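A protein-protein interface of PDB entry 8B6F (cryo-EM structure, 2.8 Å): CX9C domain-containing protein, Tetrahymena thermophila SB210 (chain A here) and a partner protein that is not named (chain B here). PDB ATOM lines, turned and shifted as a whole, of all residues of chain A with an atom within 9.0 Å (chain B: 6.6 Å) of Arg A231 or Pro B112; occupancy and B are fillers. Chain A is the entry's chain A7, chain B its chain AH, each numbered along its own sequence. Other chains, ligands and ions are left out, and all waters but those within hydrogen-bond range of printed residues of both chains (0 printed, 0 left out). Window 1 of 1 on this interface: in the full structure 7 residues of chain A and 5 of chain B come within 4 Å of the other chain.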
ATOM      1  N   SER A 184      -3.007  17.955  12.245  1.00  0.00           N
ATOM      2  CA  SER A 184      -1.965  17.912  11.227  1.00  0.00           C
ATOM      3  C   SER A 184      -2.412  16.962  10.129  1.00  0.00           C
ATOM      4  O   SER A 184      -2.814  15.829  10.407  1.00  0.00           O
ATOM      5  CB  SER A 184      -0.628  17.450  11.808  1.00  0.00           C
ATOM      6  OG  SER A 184      -0.750  16.188  12.440  1.00  0.00           O
ATOM      7  N   ASN A 187       0.707  14.204   8.986  1.00  0.00           N
ATOM      8  CA  ASN A 187       2.145  14.254   9.235  1.00  0.00           C
ATOM      9  C   ASN A 187       2.456  13.311  10.390  1.00  0.00           C
ATOM     10  O   ASN A 187       2.185  13.619  11.552  1.00  0.00           O
ATOM     11  CB  ASN A 187       2.592  15.678   9.537  1.00  0.00           C
ATOM     12  CG  ASN A 187       4.085  15.865   9.368  1.00  0.00           C
ATOM     13  OD1 ASN A 187       4.871  14.968   9.660  1.00  0.00           O
ATOM     14  ND2 ASN A 187       4.483  17.036   8.885  1.00  0.00           N
ATOM     15  N   ASN A 190       5.218  14.613  13.176  1.00  0.00           N
ATOM     16  CA  ASN A 190       4.787  15.564  14.196  1.00  0.00           C
ATOM     17  C   ASN A 190       4.034  14.876  15.324  1.00  0.00           C
ATOM     18  O   ASN A 190       4.068  15.345  16.467  1.00  0.00           O
ATOM     19  CB  ASN A 190       3.910  16.649  13.570  1.00  0.00           C
ATOM     20  CG  ASN A 190       4.673  17.531  12.605  1.00  0.00           C
ATOM     21  OD1 ASN A 190       5.893  17.654  12.690  1.00  0.00           O
ATOM     22  ND2 ASN A 190       3.952  18.159  11.683  1.00  0.00           N
ATOM     23  N   ASP A 226      -2.986  22.887  17.608  1.00  0.00           N
ATOM     24  CA  ASP A 226      -3.229  23.955  16.639  1.00  0.00           C
ATOM     25  C   ASP A 226      -1.889  24.283  15.989  1.00  0.00           C
ATOM     26  O   ASP A 226      -1.104  25.063  16.534  1.00  0.00           O
ATOM     27  CB  ASP A 226      -3.837  25.182  17.307  1.00  0.00           C
ATOM     28  CG  ASP A 226      -4.077  26.318  16.331  1.00  0.00           C
ATOM     29  OD1 ASP A 226      -3.958  26.092  15.109  1.00  0.00           O
ATOM     30  OD2 ASP A 226      -4.381  27.439  16.788  1.00  0.00           O
ATOM     31  N   PHE A 227      -1.633  23.687  14.824  1.00  0.00           N
ATOM     32  CA  PHE A 227      -0.319  23.820  14.204  1.00  0.00           C
ATOM     33  C   PHE A 227      -0.119  25.195  13.581  1.00  0.00           C
ATOM     34  O   PHE A 227       1.021  25.658  13.465  1.00  0.00           O
ATOM     35  CB  PHE A 227      -0.120  22.712  13.169  1.00  0.00           C
ATOM     36  CG  PHE A 227       0.050  21.349  13.782  1.00  0.00           C
ATOM     37  CD1 PHE A 227      -1.043  20.653  14.271  1.00  0.00           C
ATOM     38  CD2 PHE A 227       1.305  20.773  13.886  1.00  0.00           C
ATOM     39  CE1 PHE A 227      -0.889  19.404  14.843  1.00  0.00           C
ATOM     40  CE2 PHE A 227       1.465  19.524  14.457  1.00  0.00           C
ATOM     41  CZ  PHE A 227       0.368  18.839  14.936  1.00  0.00           C
ATOM     42  N   VAL A 228      -1.196  25.857  13.162  1.00  0.00           N
ATOM     43  CA  VAL A 228      -1.072  27.226  12.664  1.00  0.00           C
ATOM     44  C   VAL A 228      -0.528  28.135  13.758  1.00  0.00           C
ATOM     45  O   VAL A 228       0.373  28.949  13.526  1.00  0.00           O
ATOM     46  CB  VAL A 228      -2.427  27.726  12.134  1.00  0.00           C
ATOM     47  CG1 VAL A 228      -2.403  29.233  11.897  1.00  0.00           C
ATOM     48  CG2 VAL A 228      -2.790  26.999  10.857  1.00  0.00           C
ATOM     49  N   LYS A 229      -1.070  28.007  14.970  1.00  0.00           N
ATOM     50  CA  LYS A 229      -0.578  28.799  16.092  1.00  0.00           C
ATOM     51  C   LYS A 229       0.800  28.325  16.541  1.00  0.00           C
ATOM     52  O   LYS A 229       1.649  29.141  16.913  1.00  0.00           O
ATOM     53  CB  LYS A 229      -1.577  28.738  17.249  1.00  0.00           C
ATOM     54  CG  LYS A 229      -1.148  29.495  18.499  1.00  0.00           C
ATOM     55  CD  LYS A 229      -0.917  30.972  18.216  1.00  0.00           C
ATOM     56  CE  LYS A 229      -0.509  31.718  19.479  1.00  0.00           C
ATOM     57  NZ  LYS A 229      -0.224  33.155  19.206  1.00  0.00           N
ATOM     58  N   ASN A 230       1.040  27.016  16.515  1.00  0.00           N
ATOM     59  CA  ASN A 230       2.313  26.426  16.925  1.00  0.00           C
ATOM     60  C   ASN A 230       2.851  25.597  15.762  1.00  0.00           C
ATOM     61  O   ASN A 230       2.643  24.385  15.695  1.00  0.00           O
ATOM     62  CB  ASN A 230       2.127  25.578  18.177  1.00  0.00           C
ATOM     63  CG  ASN A 230       1.306  26.280  19.237  1.00  0.00           C
ATOM     64  OD1 ASN A 230       1.401  27.493  19.408  1.00  0.00           O
ATOM     65  ND2 ASN A 230       0.492  25.516  19.956  1.00  0.00           N
ATOM     66  N   ARG A 231       3.550  26.266  14.842  1.00  0.00           N
ATOM     67  CA  ARG A 231       4.163  25.560  13.721  1.00  0.00           C
ATOM     68  C   ARG A 231       5.188  24.536  14.192  1.00  0.00           C
ATOM     69  O   ARG A 231       5.235  23.412  13.676  1.00  0.00           O
ATOM     70  CB  ARG A 231       4.814  26.560  12.765  1.00  0.00           C
ATOM     71  CG  ARG A 231       3.822  27.390  11.967  1.00  0.00           C
ATOM     72  CD  ARG A 231       4.122  28.872  12.074  1.00  0.00           C
ATOM     73  NE  ARG A 231       3.768  29.396  13.386  1.00  0.00           N
ATOM     74  CZ  ARG A 231       4.055  30.618  13.810  1.00  0.00           C
ATOM     75  NH1 ARG A 231       4.725  31.472  13.054  1.00  0.00           N
ATOM     76  NH2 ARG A 231       3.661  30.993  15.023  1.00  0.00           N
ATOM     77  N   GLY A 232       6.019  24.903  15.164  1.00  0.00           N
ATOM     78  CA  GLY A 232       7.085  24.034  15.622  1.00  0.00           C
ATOM     79  C   GLY A 232       8.452  24.599  15.303  1.00  0.00           C
ATOM     80  O   GLY A 232       8.638  25.819  15.304  1.00  0.00           O
ATOM     81  N   HIS A 233       9.419  23.725  15.022  1.00  0.00           N
ATOM     82  CA  HIS A 233      10.788  24.129  14.714  1.00  0.00           C
ATOM     83  C   HIS A 233      11.162  23.610  13.333  1.00  0.00           C
ATOM     84  O   HIS A 233      11.330  22.401  13.145  1.00  0.00           O
ATOM     85  CB  HIS A 233      11.765  23.615  15.769  1.00  0.00           C
ATOM     86  CG  HIS A 233      11.583  24.242  17.115  1.00  0.00           C
ATOM     87  ND1 HIS A 233      10.480  24.001  17.907  1.00  0.00           N
ATOM     88  CD2 HIS A 233      12.360  25.107  17.809  1.00  0.00           C
ATOM     89  CE1 HIS A 233      10.589  24.688  19.029  1.00  0.00           C
ATOM     90  NE2 HIS A 233      11.720  25.367  18.996  1.00  0.00           N
ATOM     91  N   SER A 234      11.301  24.525  12.377  1.00  0.00           N
ATOM     92  CA  SER A 234      11.803  24.201  11.044  1.00  0.00           C
ATOM     93  C   SER A 234      11.020  23.050  10.417  1.00  0.00           C
ATOM     94  O   SER A 234      11.584  22.118   9.843  1.00  0.00           O
ATOM     95  CB  SER A 234      13.297  23.876  11.102  1.00  0.00           C
ATOM     96  OG  SER A 234      13.793  23.523   9.825  1.00  0.00           O
ATOM     97  N   ASP A 235       9.696  23.125  10.527  1.00  0.00           N
ATOM     98  CA  ASP A 235       8.828  22.075  10.002  1.00  0.00           C
ATOM     99  C   ASP A 235       8.793  22.163   8.482  1.00  0.00           C
ATOM    100  O   ASP A 235       8.303  23.148   7.919  1.00  0.00           O
ATOM    101  CB  ASP A 235       7.427  22.206  10.589  1.00  0.00           C
ATOM    102  CG  ASP A 235       6.523  21.053  10.204  1.00  0.00           C
ATOM    103  OD1 ASP A 235       7.003  20.121   9.526  1.00  0.00           O
ATOM    104  OD2 ASP A 235       5.332  21.075  10.579  1.00  0.00           O
ATOM    105  N   LYS A 236       9.315  21.136   7.814  1.00  0.00           N
ATOM    106  CA  LYS A 236       9.279  21.063   6.360  1.00  0.00           C
ATOM    107  C   LYS A 236       7.957  20.518   5.835  1.00  0.00           C
ATOM    108  O   LYS A 236       7.699  20.617   4.632  1.00  0.00           O
ATOM    109  CB  LYS A 236      10.430  20.192   5.852  1.00  0.00           C
ATOM    110  CG  LYS A 236      10.507  20.075   4.336  1.00  0.00           C
ATOM    111  CD  LYS A 236      11.684  19.221   3.912  1.00  0.00           C
ATOM    112  CE  LYS A 236      11.686  19.004   2.412  1.00  0.00           C
ATOM    113  NZ  LYS A 236      12.791  18.095   1.992  1.00  0.00           N
ATOM    114  N   TYR A 237       7.109  19.971   6.704  1.00  0.00           N
ATOM    115  CA  TYR A 237       5.892  19.284   6.279  1.00  0.00           C
ATOM    116  C   TYR A 237       6.222  18.132   5.332  1.00  0.00           C
ATOM    117  O   TYR A 237       5.517  17.875   4.357  1.00  0.00           O
ATOM    118  CB  TYR A 237       4.907  20.263   5.637  1.00  0.00           C
ATOM    119  CG  TYR A 237       4.643  21.467   6.506  1.00  0.00           C
ATOM    120  CD1 TYR A 237       3.914  21.349   7.682  1.00  0.00           C
ATOM    121  CD2 TYR A 237       5.128  22.719   6.158  1.00  0.00           C
ATOM    122  CE1 TYR A 237       3.672  22.448   8.486  1.00  0.00           C
ATOM    123  CE2 TYR A 237       4.892  23.823   6.954  1.00  0.00           C
ATOM    124  CZ  TYR A 237       4.162  23.680   8.117  1.00  0.00           C
ATOM    125  OH  TYR A 237       3.923  24.773   8.916  1.00  0.00           O
ATOM    126  N   MET B 109      -1.448  35.244   1.520  1.00  0.00           N
ATOM    127  CA  MET B 109      -1.395  34.270   2.601  1.00  0.00           C
ATOM    128  C   MET B 109      -1.223  34.991   3.929  1.00  0.00           C
ATOM    129  O   MET B 109      -0.467  35.963   4.026  1.00  0.00           O
ATOM    130  CB  MET B 109      -0.257  33.269   2.407  1.00  0.00           C
ATOM    131  CG  MET B 109      -0.445  32.370   1.197  1.00  0.00           C
ATOM    132  SD  MET B 109       0.410  30.790   1.343  1.00  0.00           S
ATOM    133  CE  MET B 109      -0.482  30.058   2.714  1.00  0.00           C
ATOM    134  N   TRP B 110      -1.930  34.506   4.948  1.00  0.00           N
ATOM    135  CA  TRP B 110      -1.924  35.116   6.272  1.00  0.00           C
ATOM    136  C   TRP B 110      -1.562  34.092   7.341  1.00  0.00           C
ATOM    137  O   TRP B 110      -2.012  34.191   8.484  1.00  0.00           O
ATOM    138  CB  TRP B 110      -3.282  35.750   6.575  1.00  0.00           C
ATOM    139  CG  TRP B 110      -3.730  36.700   5.514  1.00  0.00           C
ATOM    140  CD1 TRP B 110      -4.636  36.455   4.525  1.00  0.00           C
ATOM    141  CD2 TRP B 110      -3.286  38.048   5.328  1.00  0.00           C
ATOM    142  NE1 TRP B 110      -4.786  37.568   3.735  1.00  0.00           N
ATOM    143  CE2 TRP B 110      -3.967  38.560   4.208  1.00  0.00           C
ATOM    144  CE3 TRP B 110      -2.379  38.870   6.002  1.00  0.00           C
ATOM    145  CZ2 TRP B 110      -3.771  39.858   3.745  1.00  0.00           C
ATOM    146  CZ3 TRP B 110      -2.185  40.159   5.543  1.00  0.00           C
ATOM    147  CH2 TRP B 110      -2.878  40.641   4.424  1.00  0.00           C
ATOM    148  N   GLY B 111      -0.743  33.110   6.982  1.00  0.00           N
ATOM    149  CA  GLY B 111      -0.367  32.051   7.886  1.00  0.00           C
ATOM    150  C   GLY B 111       0.218  30.881   7.126  1.00  0.00           C
ATOM    151  O   GLY B 111       0.401  30.938   5.906  1.00  0.00           O
ATOM    152  N   PRO B 112       0.520  29.788   7.829  1.00  0.00           N
ATOM    153  CA  PRO B 112       1.107  28.630   7.136  1.00  0.00           C
ATOM    154  C   PRO B 112       0.263  28.136   5.973  1.00  0.00           C
ATOM    155  O   PRO B 112       0.812  27.790   4.920  1.00  0.00           O
ATOM    156  CB  PRO B 112       1.220  27.581   8.252  1.00  0.00           C
ATOM    157  CG  PRO B 112       1.281  28.370   9.510  1.00  0.00           C
ATOM    158  CD  PRO B 112       0.422  29.574   9.281  1.00  0.00           C
ATOM    159  N   SER B 113      -1.061  28.088   6.135  1.00  0.00           N
ATOM    160  CA  SER B 113      -1.956  27.723   5.044  1.00  0.00           C
ATOM    161  C   SER B 113      -3.220  28.572   5.058  1.00  0.00           C
ATOM    162  O   SER B 113      -4.271  28.137   4.574  1.00  0.00           O
ATOM    163  CB  SER B 113      -2.310  26.241   5.100  1.00  0.00           C
ATOM    164  OG  SER B 113      -1.141  25.463   4.919  1.00  0.00           O
ATOM    165  N   VAL B 114      -3.137  29.779   5.606  1.00  0.00           N
ATOM    166  CA  VAL B 114      -4.322  30.639   5.761  1.00  0.00           C
ATOM    167  C   VAL B 114      -4.433  31.437   4.468  1.00  0.00           C
ATOM    168  O   VAL B 114      -3.967  32.570   4.341  1.00  0.00           O
ATOM    169  CB  VAL B 114      -4.228  31.529   7.003  1.00  0.00           C
ATOM    170  CG1 VAL B 114      -5.522  32.298   7.205  1.00  0.00           C
ATOM    171  CG2 VAL B 114      -3.897  30.696   8.233  1.00  0.00           C
ATOM    172  N   SER B 115      -5.074  30.822   3.478  1.00  0.00           N
ATOM    173  CA  SER B 115      -5.335  31.458   2.198  1.00  0.00           C
ATOM    174  C   SER B 115      -6.739  31.084   1.749  1.00  0.00           C
ATOM    175  O   SER B 115      -7.213  29.978   2.011  1.00  0.00           O
ATOM    176  CB  SER B 115      -4.312  31.030   1.140  1.00  0.00           C
ATOM    177  OG  SER B 115      -4.531  31.697  -0.089  1.00  0.00           O
ATOM    178  N   CYS B 182       5.137  28.975  -3.635  1.00  0.00           N
ATOM    179  CA  CYS B 182       4.227  29.266  -2.538  1.00  0.00           C
ATOM    180  C   CYS B 182       4.911  30.129  -1.487  1.00  0.00           C
ATOM    181  O   CYS B 182       6.088  29.938  -1.173  1.00  0.00           O
ATOM    182  CB  CYS B 182       3.730  27.967  -1.901  1.00  0.00           C
ATOM    183  SG  CYS B 182       2.488  28.201  -0.612  1.00  0.00           S
ATOM    184  N   PHE B 183       4.158  31.083  -0.940  1.00  0.00           N
ATOM    185  CA  PHE B 183       4.714  31.982   0.065  1.00  0.00           C
ATOM    186  C   PHE B 183       5.052  31.259   1.364  1.00  0.00           C
ATOM    187  O   PHE B 183       5.963  31.681   2.083  1.00  0.00           O
ATOM    188  CB  PHE B 183       3.734  33.120   0.347  1.00  0.00           C
ATOM    189  CG  PHE B 183       3.486  34.024  -0.826  1.00  0.00           C
ATOM    190  CD1 PHE B 183       4.494  34.305  -1.734  1.00  0.00           C
ATOM    191  CD2 PHE B 183       2.245  34.608  -1.007  1.00  0.00           C
ATOM    192  CE1 PHE B 183       4.263  35.142  -2.807  1.00  0.00           C
ATOM    193  CE2 PHE B 183       2.008  35.446  -2.077  1.00  0.00           C
ATOM    194  CZ  PHE B 183       3.020  35.715  -2.977  1.00  0.00           C
ATOM    195  N   SER B 184       4.334  30.182   1.685  1.00  0.00           N
ATOM    196  CA  SER B 184       4.540  29.518   2.969  1.00  0.00           C
ATOM    197  C   SER B 184       5.947  28.949   3.088  1.00  0.00           C
ATOM    198  O   SER B 184       6.565  29.016   4.156  1.00  0.00           O
ATOM    199  CB  SER B 184       3.509  28.407   3.151  1.00  0.00           C
ATOM    200  OG  SER B 184       2.194  28.920   3.103  1.00  0.00           O
ATOM    201  N   VAL B 185       6.471  28.383   2.000  1.00  0.00           N
ATOM    202  CA  VAL B 185       7.745  27.677   2.056  1.00  0.00           C
ATOM    203  C   VAL B 185       8.897  28.601   2.422  1.00  0.00           C
ATOM    204  O   VAL B 185       9.961  28.124   2.830  1.00  0.00           O
ATOM    205  CB  VAL B 185       7.984  26.936   0.726  1.00  0.00           C
ATOM    206  CG1 VAL B 185       9.279  26.145   0.764  1.00  0.00           C
ATOM    207  CG2 VAL B 185       6.811  25.994   0.473  1.00  0.00           C
ATOM    208  N   VAL B 187       8.815  30.994   4.869  1.00  0.00           N
ATOM    209  CA  VAL B 187       8.852  31.275   6.300  1.00  0.00           C
ATOM    210  C   VAL B 187       9.549  30.151   7.058  1.00  0.00           C
ATOM    211  O   VAL B 187      10.253  30.395   8.043  1.00  0.00           O
ATOM    212  CB  VAL B 187       7.429  31.523   6.831  1.00  0.00           C
ATOM    213  CG1 VAL B 187       7.450  31.716   8.339  1.00  0.00           C
ATOM    214  CG2 VAL B 187       6.829  32.738   6.148  1.00  0.00           C
ATOM    215  N   GLU B 191      12.663  31.057   9.635  1.00  0.00           N
ATOM    216  CA  GLU B 191      12.438  31.008  11.076  1.00  0.00           C
ATOM    217  C   GLU B 191      13.686  31.427  11.847  1.00  0.00           C
ATOM    218  O   GLU B 191      13.614  32.255  12.761  1.00  0.00           O
ATOM    219  CB  GLU B 191      11.997  29.604  11.494  1.00  0.00           C
ATOM    220  CG  GLU B 191      10.625  29.203  10.967  1.00  0.00           C
ATOM    221  CD  GLU B 191      10.114  27.915  11.586  1.00  0.00           C
ATOM    222  OE1 GLU B 191      10.834  27.331  12.421  1.00  0.00           O
ATOM    223  OE2 GLU B 191       8.993  27.489  11.236  1.00  0.00           O
ATOM    224  N   TRP B 267       5.629  35.983   8.974  1.00  0.00           N
ATOM    225  CA  TRP B 267       4.972  35.977  10.275  1.00  0.00           C
ATOM    226  C   TRP B 267       5.864  35.406  11.372  1.00  0.00           C
ATOM    227  O   TRP B 267       5.359  34.876  12.368  1.00  0.00           O
ATOM    228  CB  TRP B 267       3.658  35.202  10.195  1.00  0.00           C
ATOM    229  CG  TRP B 267       3.772  33.866   9.523  1.00  0.00           C
ATOM    230  CD1 TRP B 267       4.153  32.691  10.098  1.00  0.00           C
ATOM    231  CD2 TRP B 267       3.502  33.571   8.148  1.00  0.00           C
ATOM    232  NE1 TRP B 267       4.137  31.682   9.167  1.00  0.00           N
ATOM    233  CE2 TRP B 267       3.742  32.197   7.961  1.00  0.00           C
ATOM    234  CE3 TRP B 267       3.081  34.338   7.057  1.00  0.00           C
ATOM    235  CZ2 TRP B 267       3.574  31.571   6.728  1.00  0.00           C
ATOM    236  CZ3 TRP B 267       2.916  33.716   5.833  1.00  0.00           C
ATOM    237  CH2 TRP B 267       3.163  32.345   5.678  1.00  0.00           C
ATOM    238  N   GLU B 268       7.179  35.505  11.210  1.00  0.00           N
ATOM    239  CA  GLU B 268       8.137  35.071  12.218  1.00  0.00           C
ATOM    240  C   GLU B 268       8.777  36.291  12.863  1.00  0.00           C
ATOM    241  O   GLU B 268       9.235  37.200  12.164  1.00  0.00           O
ATOM    242  CB  GLU B 268       9.211  34.173  11.600  1.00  0.00           C
ATOM    243  CG  GLU B 268       8.741  32.758  11.307  1.00  0.00           C
ATOM    244  CD  GLU B 268       8.454  31.962  12.567  1.00  0.00           C
ATOM    245  OE1 GLU B 268       8.772  32.454  13.669  1.00  0.00           O
ATOM    246  OE2 GLU B 268       7.908  30.845  12.456  1.00  0.00           O
ATOM    247  N   LEU B 269       8.810  36.303  14.193  1.00  0.00           N
ATOM    248  CA  LEU B 269       9.400  37.411  14.921  1.00  0.00           C
ATOM    249  C   LEU B 269      10.906  37.456  14.683  1.00  0.00           C
ATOM    250  O   LEU B 269      11.522  36.445  14.340  1.00  0.00           O
ATOM    251  CB  LEU B 269       9.108  37.282  16.413  1.00  0.00           C
ATOM    252  CG  LEU B 269       7.677  37.603  16.853  1.00  0.00           C
ATOM    253  CD1 LEU B 269       7.471  37.221  18.307  1.00  0.00           C
ATOM    254  CD2 LEU B 269       7.364  39.075  16.644  1.00  0.00           C
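Among the printed residues, pairs that only touch across the chains: Val A228 with Pro B112 (3.9 Å), Arg A231 with Pro B112 (3.7 Å), Arg A231 with Trp B267 (3.2 Å), Gly A232 with Glu B191 (3.9 Å), His A233 with Glu B191 (3.8 Å) and Tyr A237 with Pro B112 (3.95 Å).
OG of Ser B184 is in hydrogen-bond range of O of Pro B112 (2.5 Å).
The backbone NH (N) of Val A228 lies close to the side-chain carboxylate (OD1) of Asp A226 (3.4 Å).
The backbone carbonyl oxygen (O) of Val A228 lies within hydrogen-bond range of the guanidinium group (NE) of Arg A231, at 3.4 Å.
NH2 of Arg A231 lies within hydrogen-bond range of O of Lys A229 (3.3 Å).
The backbone NH (N) of Tyr A237 lies within hydrogen-bond range of the side-chain carboxylate (OD1) of Asp A235.
Printed residues of chain A that touch a printed residue of chain B: Val A228, Arg A231, Gly A232, His A233, Ser A234 and Tyr A237.
Hydrophobic or aromatic side chains of chain A within 4 Å of the printed part of chain B: Val A228 and Tyr A237.
Among the printed residues, 8 pairs touch across the chains.
Of the printed residues of chain A, Pro B112 touches Val A228, Arg A231 and Tyr A237.
No residue of chain A comes within 4 Å of Ser B113.
Of the printed residues of chain B, Gly A232 touches Glu B191 (3.9 Å).
Printed residues of chain B within 4 Å of His A233: Glu B191.
Of the printed residues of chain B, Tyr A237 touches Pro B112.
Of the printed residues of chain A, Glu B268 touches Arg A231 (3.3 Å).
Of the printed residues of chain B, Val A228 touches Pro B112 (3.9 Å).
Val B187 touches none of the printed residues of chain A.
Lys A229 touches none of the printed residues of chain B.
The nearest residue of chain A that does not touch Pro B112 is Phe A227 (4.8 Å).
The side-chain carboxylate (OE1) of Glu B191 sits at hydrogen-bond distance from the backbone NH (N) of Ser A234 (2.8 Å).
The side-chain carboxylate (OE2) of Glu B268 is in salt-bridge range of the guanidinium group (NH1) of Arg A231 (3.3 Å).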
